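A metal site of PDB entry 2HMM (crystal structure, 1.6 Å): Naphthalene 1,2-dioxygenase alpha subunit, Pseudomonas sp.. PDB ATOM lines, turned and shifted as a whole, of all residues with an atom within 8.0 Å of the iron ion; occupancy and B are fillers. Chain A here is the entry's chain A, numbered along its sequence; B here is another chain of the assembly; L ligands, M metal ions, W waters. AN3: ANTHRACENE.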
ATOM      1  N   ASN A 201      -1.876 -20.089  28.443  1.00  0.00           N
ATOM      2  CA  ASN A 201      -1.971 -18.661  28.676  1.00  0.00           C
ATOM      3  C   ASN A 201      -3.188 -18.157  27.928  1.00  0.00           C
ATOM      4  O   ASN A 201      -4.025 -17.481  28.493  1.00  0.00           O
ATOM      5  CB  ASN A 201      -0.688 -17.966  28.181  1.00  0.00           C
ATOM      6  CG  ASN A 201      -0.727 -16.468  28.360  1.00  0.00           C
ATOM      7  OD1 ASN A 201      -0.415 -15.938  29.430  1.00  0.00           O
ATOM      8  ND2 ASN A 201      -1.159 -15.779  27.325  1.00  0.00           N
ATOM      9  N   PHE A 202      -3.307 -18.528  26.654  1.00  0.00           N
ATOM     10  CA  PHE A 202      -4.483 -18.136  25.877  1.00  0.00           C
ATOM     11  C   PHE A 202      -5.775 -18.793  26.347  1.00  0.00           C
ATOM     12  O   PHE A 202      -6.829 -18.177  26.207  1.00  0.00           O
ATOM     13  CB  PHE A 202      -4.285 -18.412  24.379  1.00  0.00           C
ATOM     14  CG  PHE A 202      -3.525 -17.318  23.671  1.00  0.00           C
ATOM     15  CD1 PHE A 202      -2.206 -17.045  24.009  1.00  0.00           C
ATOM     16  CD2 PHE A 202      -4.106 -16.580  22.658  1.00  0.00           C
ATOM     17  CE1 PHE A 202      -1.496 -16.047  23.382  1.00  0.00           C
ATOM     18  CE2 PHE A 202      -3.375 -15.565  22.006  1.00  0.00           C
ATOM     19  CZ  PHE A 202      -2.063 -15.309  22.400  1.00  0.00           C
ATOM     20  N   ASP A 205      -5.860 -17.280  30.845  1.00  0.00           N
ATOM     21  CA  ASP A 205      -5.024 -16.448  31.661  1.00  0.00           C
ATOM     22  C   ASP A 205      -5.353 -14.963  31.504  1.00  0.00           C
ATOM     23  O   ASP A 205      -4.712 -14.272  30.801  1.00  0.00           O
ATOM     24  CB  ASP A 205      -3.555 -16.733  31.394  1.00  0.00           C
ATOM     25  CG  ASP A 205      -2.616 -16.130  32.427  1.00  0.00           C
ATOM     26  OD1 ASP A 205      -3.009 -15.199  33.097  1.00  0.00           O
ATOM     27  OD2 ASP A 205      -1.482 -16.531  32.466  1.00  0.00           O
ATOM     28  N   HIS A 208      -2.754 -12.406  34.040  1.00  0.00           N
ATOM     29  CA  HIS A 208      -1.452 -11.862  33.676  1.00  0.00           C
ATOM     30  C   HIS A 208      -1.554 -10.512  32.965  1.00  0.00           C
ATOM     31  O   HIS A 208      -0.575  -9.757  32.940  1.00  0.00           O
ATOM     32  CB  HIS A 208      -0.655 -12.863  32.814  1.00  0.00           C
ATOM     33  CG  HIS A 208      -0.967 -12.819  31.352  1.00  0.00           C
ATOM     34  ND1 HIS A 208      -2.158 -13.263  30.809  1.00  0.00           N
ATOM     35  CD2 HIS A 208      -0.211 -12.394  30.295  1.00  0.00           C
ATOM     36  CE1 HIS A 208      -2.128 -13.096  29.494  1.00  0.00           C
ATOM     37  NE2 HIS A 208      -0.963 -12.559  29.162  1.00  0.00           N
ATOM     38  N   VAL A 209      -2.718 -10.207  32.393  1.00  0.00           N
ATOM     39  CA  VAL A 209      -2.803  -9.140  31.390  1.00  0.00           C
ATOM     40  C   VAL A 209      -2.354  -7.794  31.919  1.00  0.00           C
ATOM     41  O   VAL A 209      -1.466  -7.173  31.314  1.00  0.00           O
ATOM     42  CB  VAL A 209      -4.199  -9.044  30.758  1.00  0.00           C
ATOM     43  CG1 VAL A 209      -4.269  -7.819  29.821  1.00  0.00           C
ATOM     44  CG2 VAL A 209      -4.489 -10.324  30.003  1.00  0.00           C
ATOM     45  N   THR A 212       1.808  -8.349  33.065  1.00  0.00           N
ATOM     46  CA  THR A 212       2.655  -8.740  31.915  1.00  0.00           C
ATOM     47  C   THR A 212       2.604  -7.674  30.816  1.00  0.00           C
ATOM     48  O   THR A 212       3.640  -7.250  30.315  1.00  0.00           O
ATOM     49  CB  THR A 212       2.257 -10.102  31.319  1.00  0.00           C
ATOM     50  OG1 THR A 212       2.554 -11.173  32.225  1.00  0.00           O
ATOM     51  CG2 THR A 212       2.983 -10.367  29.988  1.00  0.00           C
ATOM     52  N   HIS A 213       1.397  -7.227  30.495  1.00  0.00           N
ATOM     53  CA  HIS A 213       1.185  -6.301  29.382  1.00  0.00           C
ATOM     54  C   HIS A 213       1.058  -4.846  29.810  1.00  0.00           C
ATOM     55  O   HIS A 213       0.604  -4.012  29.047  1.00  0.00           O
ATOM     56  CB  HIS A 213      -0.013  -6.752  28.521  1.00  0.00           C
ATOM     57  CG  HIS A 213       0.187  -8.083  27.878  1.00  0.00           C
ATOM     58  ND1 HIS A 213       1.118  -8.297  26.880  1.00  0.00           N
ATOM     59  CD2 HIS A 213      -0.426  -9.277  28.070  1.00  0.00           C
ATOM     60  CE1 HIS A 213       1.093  -9.562  26.518  1.00  0.00           C
ATOM     61  NE2 HIS A 213       0.156 -10.183  27.206  1.00  0.00           N
ATOM     62  N   LEU A 307      -7.800 -14.930  19.802  1.00  0.00           N
ATOM     63  CA  LEU A 307      -8.485 -13.839  20.501  1.00  0.00           C
ATOM     64  C   LEU A 307      -9.507 -13.319  19.523  1.00  0.00           C
ATOM     65  O   LEU A 307      -9.156 -12.678  18.549  1.00  0.00           O
ATOM     66  CB  LEU A 307      -7.515 -12.730  20.866  1.00  0.00           C
ATOM     67  CG  LEU A 307      -6.299 -13.024  21.751  1.00  0.00           C
ATOM     68  CD1 LEU A 307      -5.476 -11.750  21.973  1.00  0.00           C
ATOM     69  CD2 LEU A 307      -6.667 -13.755  23.067  1.00  0.00           C
ATOM     70  N   PHE A 352       0.482  -8.775  17.997  1.00  0.00           N
ATOM     71  CA  PHE A 352       0.719 -10.170  18.317  1.00  0.00           C
ATOM     72  C   PHE A 352       1.512 -10.976  17.283  1.00  0.00           C
ATOM     73  O   PHE A 352       1.662 -12.181  17.434  1.00  0.00           O
ATOM     74  CB  PHE A 352      -0.618 -10.859  18.603  1.00  0.00           C
ATOM     75  CG  PHE A 352      -1.066 -10.667  19.998  1.00  0.00           C
ATOM     76  CD1 PHE A 352      -1.809  -9.561  20.342  1.00  0.00           C
ATOM     77  CD2 PHE A 352      -0.692 -11.547  20.987  1.00  0.00           C
ATOM     78  CE1 PHE A 352      -2.192  -9.364  21.651  1.00  0.00           C
ATOM     79  CE2 PHE A 352      -1.054 -11.354  22.304  1.00  0.00           C
ATOM     80  CZ  PHE A 352      -1.821 -10.259  22.631  1.00  0.00           C
ATOM     81  N   TRP A 358       2.747  -6.626  22.094  1.00  0.00           N
ATOM     82  CA  TRP A 358       2.079  -7.357  23.186  1.00  0.00           C
ATOM     83  C   TRP A 358       2.708  -8.739  23.330  1.00  0.00           C
ATOM     84  O   TRP A 358       3.093  -9.139  24.420  1.00  0.00           O
ATOM     85  CB  TRP A 358       0.579  -7.528  22.927  1.00  0.00           C
ATOM     86  CG  TRP A 358      -0.223  -6.279  23.004  1.00  0.00           C
ATOM     87  CD1 TRP A 358      -0.143  -5.195  22.190  1.00  0.00           C
ATOM     88  CD2 TRP A 358      -1.326  -6.041  23.888  1.00  0.00           C
ATOM     89  NE1 TRP A 358      -1.131  -4.284  22.515  1.00  0.00           N
ATOM     90  CE2 TRP A 358      -1.853  -4.767  23.574  1.00  0.00           C
ATOM     91  CE3 TRP A 358      -1.900  -6.766  24.938  1.00  0.00           C
ATOM     92  CZ2 TRP A 358      -2.935  -4.215  24.260  1.00  0.00           C
ATOM     93  CZ3 TRP A 358      -3.002  -6.230  25.601  1.00  0.00           C
ATOM     94  CH2 TRP A 358      -3.490  -4.953  25.274  1.00  0.00           C
ATOM     95  N   GLU A 359       2.807  -9.452  22.222  1.00  0.00           N
ATOM     96  CA  GLU A 359       3.331 -10.819  22.211  1.00  0.00           C
ATOM     97  C   GLU A 359       4.732 -10.854  22.830  1.00  0.00           C
ATOM     98  O   GLU A 359       5.063 -11.769  23.604  1.00  0.00           O
ATOM     99  CB  GLU A 359       3.324 -11.363  20.765  1.00  0.00           C
ATOM    100  CG  GLU A 359       3.944 -12.743  20.563  1.00  0.00           C
ATOM    101  CD  GLU A 359       2.941 -13.880  20.489  1.00  0.00           C
ATOM    102  OE1 GLU A 359       1.801 -13.735  20.981  1.00  0.00           O
ATOM    103  OE2 GLU A 359       3.316 -14.939  19.945  1.00  0.00           O
ATOM    104  N   SER A 360       5.522  -9.821  22.556  1.00  0.00           N
ATOM    105  CA  SER A 360       6.869  -9.757  23.101  1.00  0.00           C
ATOM    106  C   SER A 360       6.885  -9.718  24.621  1.00  0.00           C
ATOM    107  O   SER A 360       7.804 -10.272  25.255  1.00  0.00           O
ATOM    108  CB  SER A 360       7.643  -8.566  22.526  1.00  0.00           C
ATOM    109  OG  SER A 360       7.328  -7.325  23.144  1.00  0.00           O
ATOM    110  N   ASP A 361       5.884  -9.085  25.221  1.00  0.00           N
ATOM    111  CA  ASP A 361       5.760  -9.050  26.685  1.00  0.00           C
ATOM    112  C   ASP A 361       5.712 -10.452  27.286  1.00  0.00           C
ATOM    113  O   ASP A 361       6.128 -10.652  28.419  1.00  0.00           O
ATOM    114  CB  ASP A 361       4.475  -8.339  27.110  1.00  0.00           C
ATOM    115  CG  ASP A 361       4.401  -6.869  26.677  1.00  0.00           C
ATOM    116  OD1 ASP A 361       5.469  -6.204  26.419  1.00  0.00           O
ATOM    117  OD2 ASP A 361       3.238  -6.390  26.541  1.00  0.00           O
ATOM    118  N   ASP A 362       5.145 -11.405  26.550  1.00  0.00           N
ATOM    119  CA  ASP A 362       4.930 -12.762  27.058  1.00  0.00           C
ATOM    120  C   ASP A 362       6.176 -13.638  26.951  1.00  0.00           C
ATOM    121  O   ASP A 362       6.212 -14.693  27.576  1.00  0.00           O
ATOM    122  CB  ASP A 362       3.819 -13.444  26.283  1.00  0.00           C
ATOM    123  CG  ASP A 362       2.450 -12.901  26.598  1.00  0.00           C
ATOM    124  OD1 ASP A 362       2.011 -13.007  27.758  1.00  0.00           O
ATOM    125  OD2 ASP A 362       1.793 -12.444  25.648  1.00  0.00           O
ATOM    126  N   ASN A 363       7.178 -13.231  26.163  1.00  0.00           N
ATOM    127  CA  ASN A 363       8.302 -14.141  25.793  1.00  0.00           C
ATOM    128  C   ASN A 363       9.016 -14.708  26.979  1.00  0.00           C
ATOM    129  O   ASN A 363       9.146 -15.917  27.062  1.00  0.00           O
ATOM    130  CB  ASN A 363       9.392 -13.436  24.956  1.00  0.00           C
ATOM    131  CG  ASN A 363       9.042 -13.254  23.487  1.00  0.00           C
ATOM    132  OD1 ASN A 363       9.848 -12.636  22.750  1.00  0.00           O
ATOM    133  ND2 ASN A 363       7.901 -13.785  23.036  1.00  0.00           N
ATOM    134  N   ASN A 365       8.280 -14.788  30.117  1.00  0.00           N
ATOM    135  CA  ASN A 365       7.352 -15.569  30.936  1.00  0.00           C
ATOM    136  C   ASN A 365       7.237 -16.984  30.425  1.00  0.00           C
ATOM    137  O   ASN A 365       7.426 -17.931  31.180  1.00  0.00           O
ATOM    138  CB  ASN A 365       5.965 -14.927  30.947  1.00  0.00           C
ATOM    139  CG  ASN A 365       5.918 -13.586  31.688  1.00  0.00           C
ATOM    140  OD1 ASN A 365       6.741 -13.290  32.548  1.00  0.00           O
ATOM    141  ND2 ASN A 365       4.933 -12.785  31.359  1.00  0.00           N
ATOM    142  N   MET A 366       6.952 -17.152  29.140  1.00  0.00           N
ATOM    143  CA  MET A 366       6.747 -18.489  28.538  1.00  0.00           C
ATOM    144  C   MET A 366       8.040 -19.278  28.472  1.00  0.00           C
ATOM    145  O   MET A 366       8.065 -20.478  28.758  1.00  0.00           O
ATOM    146  CB  MET A 366       6.260 -18.408  27.099  1.00  0.00           C
ATOM    147  CG  MET A 366       5.335 -17.275  26.747  1.00  0.00           C
ATOM    148  SD  MET A 366       3.707 -17.862  26.461  1.00  0.00           S
ATOM    149  CE  MET A 366       3.396 -18.447  28.080  1.00  0.00           C
ATOM    150  N   TYR B 103       5.071 -12.198  35.592  1.00  0.00           N
ATOM    151  CA  TYR B 103       4.005 -12.887  34.903  1.00  0.00           C
ATOM    152  C   TYR B 103       2.659 -12.437  35.488  1.00  0.00           C
ATOM    153  O   TYR B 103       1.931 -11.703  34.829  1.00  0.00           O
ATOM    154  CB  TYR B 103       4.233 -14.405  34.951  1.00  0.00           C
ATOM    155  CG  TYR B 103       3.499 -15.236  33.906  1.00  0.00           C
ATOM    156  CD1 TYR B 103       2.414 -14.710  33.174  1.00  0.00           C
ATOM    157  CD2 TYR B 103       3.845 -16.568  33.682  1.00  0.00           C
ATOM    158  CE1 TYR B 103       1.744 -15.475  32.256  1.00  0.00           C
ATOM    159  CE2 TYR B 103       3.184 -17.336  32.741  1.00  0.00           C
ATOM    160  CZ  TYR B 103       2.129 -16.778  32.047  1.00  0.00           C
ATOM    161  OH  TYR B 103       1.475 -17.544  31.112  1.00  0.00           O
HETATM  162  C1  AN3 L   1      -4.863 -12.031  26.269  1.00  0.00           C
HETATM  163  C2  AN3 L   1      -3.831 -12.821  25.819  1.00  0.00           C
HETATM  164  C3  AN3 L   1      -5.786 -12.497  27.157  1.00  0.00           C
HETATM  165  C4  AN3 L   1      -3.697 -14.091  26.293  1.00  0.00           C
HETATM  166  C5  AN3 L   1      -5.631 -13.770  27.638  1.00  0.00           C
HETATM  167  C6  AN3 L   1      -4.618 -14.573  27.196  1.00  0.00           C
HETATM  168  C7  AN3 L   1      -8.047  -8.307  27.038  1.00  0.00           C
HETATM  169  C8  AN3 L   1      -7.120  -7.852  26.131  1.00  0.00           C
HETATM  170  C9  AN3 L   1      -7.940  -9.591  27.513  1.00  0.00           C
HETATM  171  C10 AN3 L   1      -6.110  -8.683  25.726  1.00  0.00           C
HETATM  172  C11 AN3 L   1      -6.939 -10.428  27.088  1.00  0.00           C
HETATM  173  C12 AN3 L   1      -6.024  -9.963  26.194  1.00  0.00           C
HETATM  174  C13 AN3 L   1      -4.979 -10.750  25.804  1.00  0.00           C
HETATM  175  C14 AN3 L   1      -6.814 -11.701  27.573  1.00  0.00           C
HETATM  176 FE    FE M   1      -0.006 -12.207  27.288  1.00  0.00          FE
HETATM  177  O   HOH W   1      -0.955 -13.358  26.045  1.00  0.00           O
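The iron ion is bound by water W1 (1.9 Å), NE2 of His 213 (2.0 Å), NE2 of His 208 (2.1 Å), OD1 of Asp 362 (2.2 Å) and OD2 of Asp 362 (2.4 Å).
ND2 of Asn 201 touches the iron ion (3.8 Å).
The side-chain carboxylate of Asp 205 lies close to the side-chain amide oxygen of Asn 201 (3.3 Å).
ND1 of His 208 lies within hydrogen-bond range of O of Asp 205 (2.7 Å).
The side-chain hydroxyl (OH) of Tyr 103 of chain B is in hydrogen-bond range of the side-chain amide oxygen (OD1) of Asn 201, at 3.0 Å.
ND1 of His 213 is in hydrogen-bond range of OD2 of Asp 361, at 2.9 Å.
A ring nitrogen (ND1) of His 208 lies close to the side-chain amide oxygen (OD1) of Asn 201 (3.5 Å).
The backbone carbonyl oxygen of Trp 358 lies close to a ring nitrogen (ND1) of His 213 (3.3 Å).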
